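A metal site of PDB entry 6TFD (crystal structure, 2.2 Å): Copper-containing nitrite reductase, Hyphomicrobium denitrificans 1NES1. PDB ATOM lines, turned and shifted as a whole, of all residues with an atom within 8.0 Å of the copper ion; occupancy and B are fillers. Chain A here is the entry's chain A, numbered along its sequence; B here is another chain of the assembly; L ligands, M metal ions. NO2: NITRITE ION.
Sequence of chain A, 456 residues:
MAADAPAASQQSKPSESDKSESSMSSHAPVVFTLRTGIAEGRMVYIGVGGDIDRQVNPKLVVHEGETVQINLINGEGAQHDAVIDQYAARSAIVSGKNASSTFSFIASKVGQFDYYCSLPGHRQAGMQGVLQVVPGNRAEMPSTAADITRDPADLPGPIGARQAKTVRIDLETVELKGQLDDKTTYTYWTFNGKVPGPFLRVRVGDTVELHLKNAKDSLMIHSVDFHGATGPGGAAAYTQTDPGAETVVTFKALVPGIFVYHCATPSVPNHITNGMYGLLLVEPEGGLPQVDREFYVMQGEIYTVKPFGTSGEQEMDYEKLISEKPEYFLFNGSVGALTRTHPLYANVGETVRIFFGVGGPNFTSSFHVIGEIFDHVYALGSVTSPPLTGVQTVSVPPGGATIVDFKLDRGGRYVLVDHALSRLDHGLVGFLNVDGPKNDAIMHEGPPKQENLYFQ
The backbone NH of Asp 225 is in hydrogen-bond range of the backbone carbonyl oxygen of His 262 (2.8 Å).
A ring nitrogen (ND1) of His 227 sits at hydrogen-bond distance from the backbone carbonyl oxygen (O) of Gly 399 (3.1 Å).
A ring nitrogen (ND1) of His 227 lies within hydrogen-bond range of the side-chain amide oxygen of Gln 392 of chain B.
ND1 of His 368 of chain B lies within hydrogen-bond range of O of Gln 392 of chain B, 2.7 Å away.
The side-chain hydroxyl (OG1) of Thr 393 of chain B lies within hydrogen-bond range of a ring nitrogen (ND1) of His 368 of chain B (3.1 Å).
The backbone NH of Val 417 of chain B is in hydrogen-bond range of the backbone carbonyl oxygen of His 368 of chain B (3.0 Å).
N of His 227 sits close to O of Val 260 (3.2 Å).
Residues that only touch the copper ion: Asp 225 (3.7 Å) and His 368 of chain B (3.9 Å).
Of the 25 residues printed, 5 come within 4 Å of the copper ion.
The nearest printed residue that does not touch the copper ion is Leu 421 of chain B (5.0 Å).
O2 of the ligand is bound to the copper ion, 1.9 Å away.
NE2 of His 262 binds the copper ion (2.1 Å).
The copper ion is bound by NE2 of His 419 of chain B (2.1 Å).
A ring nitrogen (NE2) of His 227 binds the copper ion, 2.1 Å away.
The copper ion has four donor atoms within binding distance.
Slightly farther from the copper ion lies an oxygen (O1) of the ligand (2.8 Å).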
ATOM      1  N   ASP A 225     -12.687 -24.285 -24.337  1.00  0.00           N
ATOM      2  CA  ASP A 225     -11.531 -23.366 -24.525  1.00  0.00           C
ATOM      3  C   ASP A 225     -11.949 -21.993 -23.992  1.00  0.00           C
ATOM      4  O   ASP A 225     -13.034 -21.495 -24.428  1.00  0.00           O
ATOM      5  CB  ASP A 225     -11.118 -23.358 -26.002  1.00  0.00           C
ATOM      6  CG  ASP A 225     -10.256 -22.183 -26.477  1.00  0.00           C
ATOM      7  OD1 ASP A 225      -9.884 -21.345 -25.655  1.00  0.00           O
ATOM      8  OD2 ASP A 225      -9.947 -22.150 -27.681  1.00  0.00           O
ATOM      9  N   PHE A 226     -11.154 -21.442 -23.053  1.00  0.00           N
ATOM     10  CA  PHE A 226     -11.223 -20.038 -22.526  1.00  0.00           C
ATOM     11  C   PHE A 226     -10.159 -19.179 -23.232  1.00  0.00           C
ATOM     12  O   PHE A 226      -8.923 -19.512 -23.164  1.00  0.00           O
ATOM     13  CB  PHE A 226     -11.062 -19.978 -21.003  1.00  0.00           C
ATOM     14  CG  PHE A 226     -11.966 -20.886 -20.183  1.00  0.00           C
ATOM     15  CD1 PHE A 226     -13.233 -20.481 -19.801  1.00  0.00           C
ATOM     16  CD2 PHE A 226     -11.534 -22.144 -19.793  1.00  0.00           C
ATOM     17  CE1 PHE A 226     -14.064 -21.317 -19.068  1.00  0.00           C
ATOM     18  CE2 PHE A 226     -12.374 -22.987 -19.079  1.00  0.00           C
ATOM     19  CZ  PHE A 226     -13.637 -22.578 -18.721  1.00  0.00           C
ATOM     20  N   HIS A 227     -10.568 -18.090 -23.875  1.00  0.00           N
ATOM     21  CA  HIS A 227      -9.636 -17.122 -24.530  1.00  0.00           C
ATOM     22  C   HIS A 227      -8.828 -16.366 -23.456  1.00  0.00           C
ATOM     23  O   HIS A 227      -7.848 -15.686 -23.848  1.00  0.00           O
ATOM     24  CB  HIS A 227     -10.411 -16.153 -25.425  1.00  0.00           C
ATOM     25  CG  HIS A 227     -10.946 -16.806 -26.657  1.00  0.00           C
ATOM     26  ND1 HIS A 227     -11.459 -16.086 -27.721  1.00  0.00           N
ATOM     27  CD2 HIS A 227     -11.010 -18.117 -26.998  1.00  0.00           C
ATOM     28  CE1 HIS A 227     -11.830 -16.915 -28.670  1.00  0.00           C
ATOM     29  NE2 HIS A 227     -11.566 -18.173 -28.248  1.00  0.00           N
ATOM     30  N   GLY A 233      -5.001 -25.594 -26.042  1.00  0.00           N
ATOM     31  CA  GLY A 233      -6.433 -25.430 -26.342  1.00  0.00           C
ATOM     32  C   GLY A 233      -7.141 -24.389 -25.468  1.00  0.00           C
ATOM     33  O   GLY A 233      -8.398 -24.422 -25.437  1.00  0.00           O
ATOM     34  N   VAL A 260     -14.273 -14.500 -24.731  1.00  0.00           N
ATOM     35  CA  VAL A 260     -15.288 -15.555 -25.027  1.00  0.00           C
ATOM     36  C   VAL A 260     -14.650 -16.891 -24.646  1.00  0.00           C
ATOM     37  O   VAL A 260     -13.419 -17.017 -24.768  1.00  0.00           O
ATOM     38  CB  VAL A 260     -15.880 -15.571 -26.445  1.00  0.00           C
ATOM     39  CG1 VAL A 260     -15.609 -14.315 -27.251  1.00  0.00           C
ATOM     40  CG2 VAL A 260     -15.504 -16.826 -27.209  1.00  0.00           C
ATOM     41  N   TYR A 261     -15.483 -17.803 -24.146  1.00  0.00           N
ATOM     42  CA  TYR A 261     -15.170 -19.247 -23.979  1.00  0.00           C
ATOM     43  C   TYR A 261     -16.182 -20.002 -24.843  1.00  0.00           C
ATOM     44  O   TYR A 261     -17.288 -19.467 -25.067  1.00  0.00           O
ATOM     45  CB  TYR A 261     -15.181 -19.637 -22.499  1.00  0.00           C
ATOM     46  CG  TYR A 261     -16.516 -19.730 -21.800  1.00  0.00           C
ATOM     47  CD1 TYR A 261     -17.211 -20.936 -21.726  1.00  0.00           C
ATOM     48  CD2 TYR A 261     -17.056 -18.647 -21.122  1.00  0.00           C
ATOM     49  CE1 TYR A 261     -18.422 -21.043 -21.043  1.00  0.00           C
ATOM     50  CE2 TYR A 261     -18.253 -18.734 -20.421  1.00  0.00           C
ATOM     51  CZ  TYR A 261     -18.949 -19.936 -20.385  1.00  0.00           C
ATOM     52  OH  TYR A 261     -20.142 -20.036 -19.723  1.00  0.00           O
ATOM     53  N   HIS A 262     -15.794 -21.175 -25.353  1.00  0.00           N
ATOM     54  CA  HIS A 262     -16.625 -21.989 -26.277  1.00  0.00           C
ATOM     55  C   HIS A 262     -16.202 -23.449 -26.196  1.00  0.00           C
ATOM     56  O   HIS A 262     -15.037 -23.700 -25.792  1.00  0.00           O
ATOM     57  CB  HIS A 262     -16.532 -21.451 -27.717  1.00  0.00           C
ATOM     58  CG  HIS A 262     -15.172 -21.469 -28.329  1.00  0.00           C
ATOM     59  ND1 HIS A 262     -14.587 -22.639 -28.829  1.00  0.00           N
ATOM     60  CD2 HIS A 262     -14.286 -20.488 -28.575  1.00  0.00           C
ATOM     61  CE1 HIS A 262     -13.398 -22.358 -29.350  1.00  0.00           C
ATOM     62  NE2 HIS A 262     -13.188 -21.048 -29.192  1.00  0.00           N
ATOM     63  N   CYS A 263     -17.106 -24.383 -26.560  1.00  0.00           N
ATOM     64  CA  CYS A 263     -16.780 -25.818 -26.699  1.00  0.00           C
ATOM     65  C   CYS A 263     -15.711 -25.937 -27.778  1.00  0.00           C
ATOM     66  O   CYS A 263     -15.672 -25.075 -28.658  1.00  0.00           O
ATOM     67  CB  CYS A 263     -17.982 -26.722 -27.013  1.00  0.00           C
ATOM     68  SG  CYS A 263     -17.565 -28.473 -27.229  1.00  0.00           S
ATOM     69  N   ALA A 264     -14.858 -26.949 -27.688  1.00  0.00           N
ATOM     70  CA  ALA A 264     -13.690 -27.141 -28.580  1.00  0.00           C
ATOM     71  C   ALA A 264     -13.552 -28.629 -28.899  1.00  0.00           C
ATOM     72  O   ALA A 264     -12.436 -29.113 -28.941  1.00  0.00           O
ATOM     73  CB  ALA A 264     -12.434 -26.617 -27.923  1.00  0.00           C
ATOM     74  N   VAL A 268     -15.954 -28.031 -34.199  1.00  0.00           N
ATOM     75  CA  VAL A 268     -15.986 -26.847 -33.291  1.00  0.00           C
ATOM     76  C   VAL A 268     -17.036 -25.890 -33.822  1.00  0.00           C
ATOM     77  O   VAL A 268     -17.907 -25.474 -33.058  1.00  0.00           O
ATOM     78  CB  VAL A 268     -14.591 -26.202 -33.113  1.00  0.00           C
ATOM     79  CG1 VAL A 268     -14.647 -24.933 -32.262  1.00  0.00           C
ATOM     80  CG2 VAL A 268     -13.584 -27.192 -32.544  1.00  0.00           C
ATOM     81  N   ILE A 272     -20.219 -24.733 -31.601  1.00  0.00           N
ATOM     82  CA  ILE A 272     -20.481 -23.280 -31.365  1.00  0.00           C
ATOM     83  C   ILE A 272     -21.873 -22.912 -31.887  1.00  0.00           C
ATOM     84  O   ILE A 272     -22.604 -22.366 -31.090  1.00  0.00           O
ATOM     85  CB  ILE A 272     -19.398 -22.337 -31.925  1.00  0.00           C
ATOM     86  CG1 ILE A 272     -18.091 -22.409 -31.141  1.00  0.00           C
ATOM     87  CG2 ILE A 272     -19.904 -20.902 -31.932  1.00  0.00           C
ATOM     88  CD1 ILE A 272     -16.886 -21.867 -31.911  1.00  0.00           C
ATOM     89  N   GLY A 359     -20.215 -15.319 -30.214  1.00  0.00           N
ATOM     90  CA  GLY A 359     -19.893 -16.748 -30.373  1.00  0.00           C
ATOM     91  C   GLY A 359     -19.665 -17.060 -31.842  1.00  0.00           C
ATOM     92  O   GLY A 359     -18.697 -17.778 -32.165  1.00  0.00           O
ATOM     93  N   PRO A 398     -16.242 -12.812 -34.568  1.00  0.00           N
ATOM     94  CA  PRO A 398     -16.490 -14.073 -33.876  1.00  0.00           C
ATOM     95  C   PRO A 398     -15.266 -14.409 -33.020  1.00  0.00           C
ATOM     96  O   PRO A 398     -14.147 -14.135 -33.478  1.00  0.00           O
ATOM     97  CB  PRO A 398     -16.631 -15.069 -35.041  1.00  0.00           C
ATOM     98  CG  PRO A 398     -15.780 -14.450 -36.140  1.00  0.00           C
ATOM     99  CD  PRO A 398     -16.116 -12.983 -36.026  1.00  0.00           C
ATOM    100  N   GLY A 399     -15.483 -14.946 -31.821  1.00  0.00           N
ATOM    101  CA  GLY A 399     -14.400 -15.270 -30.868  1.00  0.00           C
ATOM    102  C   GLY A 399     -13.771 -13.998 -30.307  1.00  0.00           C
ATOM    103  O   GLY A 399     -12.658 -14.089 -29.752  1.00  0.00           O
ATOM    104  N   GLY A 400     -14.461 -12.869 -30.470  1.00  0.00           N
ATOM    105  CA  GLY A 400     -14.135 -11.568 -29.872  1.00  0.00           C
ATOM    106  C   GLY A 400     -15.246 -11.090 -28.936  1.00  0.00           C
ATOM    107  O   GLY A 400     -16.346 -11.648 -28.987  1.00  0.00           O
ATOM    108  N   HIS B  27      -6.382 -30.688 -33.412  1.00  0.00           N
ATOM    109  CA  HIS B  27      -7.020 -29.615 -34.228  1.00  0.00           C
ATOM    110  C   HIS B  27      -6.861 -29.946 -35.739  1.00  0.00           C
ATOM    111  O   HIS B  27      -7.326 -29.142 -36.578  1.00  0.00           O
ATOM    112  CB  HIS B  27      -6.537 -28.224 -33.784  1.00  0.00           C
ATOM    113  CG  HIS B  27      -7.648 -27.255 -33.456  1.00  0.00           C
ATOM    114  ND1 HIS B  27      -8.516 -26.735 -34.424  1.00  0.00           N
ATOM    115  CD2 HIS B  27      -8.058 -26.724 -32.271  1.00  0.00           C
ATOM    116  CE1 HIS B  27      -9.400 -25.928 -33.844  1.00  0.00           C
ATOM    117  NE2 HIS B  27      -9.142 -25.909 -32.537  1.00  0.00           N
ATOM    118  N   HIS B 368      -6.398 -15.027 -34.280  1.00  0.00           N
ATOM    119  CA  HIS B 368      -6.399 -15.564 -32.896  1.00  0.00           C
ATOM    120  C   HIS B 368      -5.385 -16.700 -32.830  1.00  0.00           C
ATOM    121  O   HIS B 368      -5.167 -17.353 -33.864  1.00  0.00           O
ATOM    122  CB  HIS B 368      -7.799 -16.055 -32.550  1.00  0.00           C
ATOM    123  CG  HIS B 368      -7.932 -16.688 -31.210  1.00  0.00           C
ATOM    124  ND1 HIS B 368      -8.016 -15.955 -30.051  1.00  0.00           N
ATOM    125  CD2 HIS B 368      -8.087 -17.994 -30.862  1.00  0.00           C
ATOM    126  CE1 HIS B 368      -8.203 -16.775 -29.034  1.00  0.00           C
ATOM    127  NE2 HIS B 368      -8.239 -18.034 -29.504  1.00  0.00           N
ATOM    128  N   VAL B 369      -4.761 -16.902 -31.684  1.00  0.00           N
ATOM    129  CA  VAL B 369      -3.844 -18.053 -31.439  1.00  0.00           C
ATOM    130  C   VAL B 369      -4.416 -18.818 -30.265  1.00  0.00           C
ATOM    131  O   VAL B 369      -4.417 -18.244 -29.146  1.00  0.00           O
ATOM    132  CB  VAL B 369      -2.394 -17.620 -31.172  1.00  0.00           C
ATOM    133  CG1 VAL B 369      -1.527 -18.790 -30.766  1.00  0.00           C
ATOM    134  CG2 VAL B 369      -1.783 -16.908 -32.369  1.00  0.00           C
ATOM    135  N   ILE B 370      -4.910 -20.026 -30.498  1.00  0.00           N
ATOM    136  CA  ILE B 370      -5.584 -20.838 -29.460  1.00  0.00           C
ATOM    137  C   ILE B 370      -4.542 -21.128 -28.379  1.00  0.00           C
ATOM    138  O   ILE B 370      -3.440 -21.595 -28.746  1.00  0.00           O
ATOM    139  CB  ILE B 370      -6.206 -22.116 -30.054  1.00  0.00           C
ATOM    140  CG1 ILE B 370      -7.248 -21.826 -31.136  1.00  0.00           C
ATOM    141  CG2 ILE B 370      -6.816 -22.989 -28.966  1.00  0.00           C
ATOM    142  CD1 ILE B 370      -7.760 -23.083 -31.823  1.00  0.00           C
ATOM    143  N   GLY B 371      -4.857 -20.801 -27.127  1.00  0.00           N
ATOM    144  CA  GLY B 371      -4.035 -21.088 -25.942  1.00  0.00           C
ATOM    145  C   GLY B 371      -3.134 -19.919 -25.550  1.00  0.00           C
ATOM    146  O   GLY B 371      -2.333 -20.075 -24.612  1.00  0.00           O
ATOM    147  N   GLN B 392      -7.653 -10.930 -27.122  1.00  0.00           N
ATOM    148  CA  GLN B 392      -7.893 -12.338 -27.535  1.00  0.00           C
ATOM    149  C   GLN B 392      -7.819 -12.449 -29.071  1.00  0.00           C
ATOM    150  O   GLN B 392      -7.161 -13.403 -29.563  1.00  0.00           O
ATOM    151  CB  GLN B 392      -9.222 -12.889 -27.028  1.00  0.00           C
ATOM    152  CG  GLN B 392     -10.468 -12.231 -27.598  1.00  0.00           C
ATOM    153  CD  GLN B 392     -11.639 -12.400 -26.659  1.00  0.00           C
ATOM    154  OE1 GLN B 392     -12.090 -13.520 -26.350  1.00  0.00           O
ATOM    155  NE2 GLN B 392     -12.131 -11.283 -26.157  1.00  0.00           N
ATOM    156  N   THR B 393      -8.441 -11.520 -29.789  1.00  0.00           N
ATOM    157  CA  THR B 393      -8.740 -11.654 -31.242  1.00  0.00           C
ATOM    158  C   THR B 393      -8.763 -10.266 -31.877  1.00  0.00           C
ATOM    159  O   THR B 393      -9.409  -9.364 -31.270  1.00  0.00           O
ATOM    160  CB  THR B 393     -10.080 -12.390 -31.397  1.00  0.00           C
ATOM    161  OG1 THR B 393     -10.009 -13.703 -30.830  1.00  0.00           O
ATOM    162  CG2 THR B 393     -10.530 -12.523 -32.831  1.00  0.00           C
ATOM    163  N   VAL B 417      -5.585 -19.336 -36.113  1.00  0.00           N
ATOM    164  CA  VAL B 417      -6.899 -19.469 -36.801  1.00  0.00           C
ATOM    165  C   VAL B 417      -7.464 -18.087 -37.156  1.00  0.00           C
ATOM    166  O   VAL B 417      -7.132 -17.093 -36.475  1.00  0.00           O
ATOM    167  CB  VAL B 417      -7.891 -20.290 -35.940  1.00  0.00           C
ATOM    168  CG1 VAL B 417      -7.308 -21.595 -35.433  1.00  0.00           C
ATOM    169  CG2 VAL B 417      -8.440 -19.468 -34.782  1.00  0.00           C
ATOM    170  N   HIS B 419     -11.118 -16.802 -36.658  1.00  0.00           N
ATOM    171  CA  HIS B 419     -12.074 -17.312 -35.646  1.00  0.00           C
ATOM    172  C   HIS B 419     -13.497 -17.324 -36.232  1.00  0.00           C
ATOM    173  O   HIS B 419     -14.433 -17.660 -35.496  1.00  0.00           O
ATOM    174  CB  HIS B 419     -11.957 -16.519 -34.341  1.00  0.00           C
ATOM    175  CG  HIS B 419     -12.286 -17.325 -33.143  1.00  0.00           C
ATOM    176  ND1 HIS B 419     -13.523 -17.920 -32.980  1.00  0.00           N
ATOM    177  CD2 HIS B 419     -11.535 -17.683 -32.077  1.00  0.00           C
ATOM    178  CE1 HIS B 419     -13.523 -18.613 -31.863  1.00  0.00           C
ATOM    179  NE2 HIS B 419     -12.315 -18.471 -31.286  1.00  0.00           N
ATOM    180  N   LEU B 421     -14.791 -19.782 -37.808  1.00  0.00           N
ATOM    181  CA  LEU B 421     -14.133 -21.110 -37.652  1.00  0.00           C
ATOM    182  C   LEU B 421     -14.574 -22.121 -38.699  1.00  0.00           C
ATOM    183  O   LEU B 421     -13.908 -23.205 -38.768  1.00  0.00           O
ATOM    184  CB  LEU B 421     -14.392 -21.618 -36.233  1.00  0.00           C
ATOM    185  CG  LEU B 421     -13.499 -20.996 -35.163  1.00  0.00           C
ATOM    186  CD1 LEU B 421     -13.925 -21.505 -33.796  1.00  0.00           C
ATOM    187  CD2 LEU B 421     -12.009 -21.240 -35.443  1.00  0.00           C
HETATM  188  N   NO2 L   1     -10.481 -20.611 -30.741  1.00  0.00           N
HETATM  189  O1  NO2 L   1     -10.764 -21.275 -31.772  1.00  0.00           O
HETATM  190  O2  NO2 L   1     -10.271 -20.846 -29.519  1.00  0.00           O
HETATM  191 CU    CU M   1     -11.753 -19.654 -29.684  1.00  0.00          CU
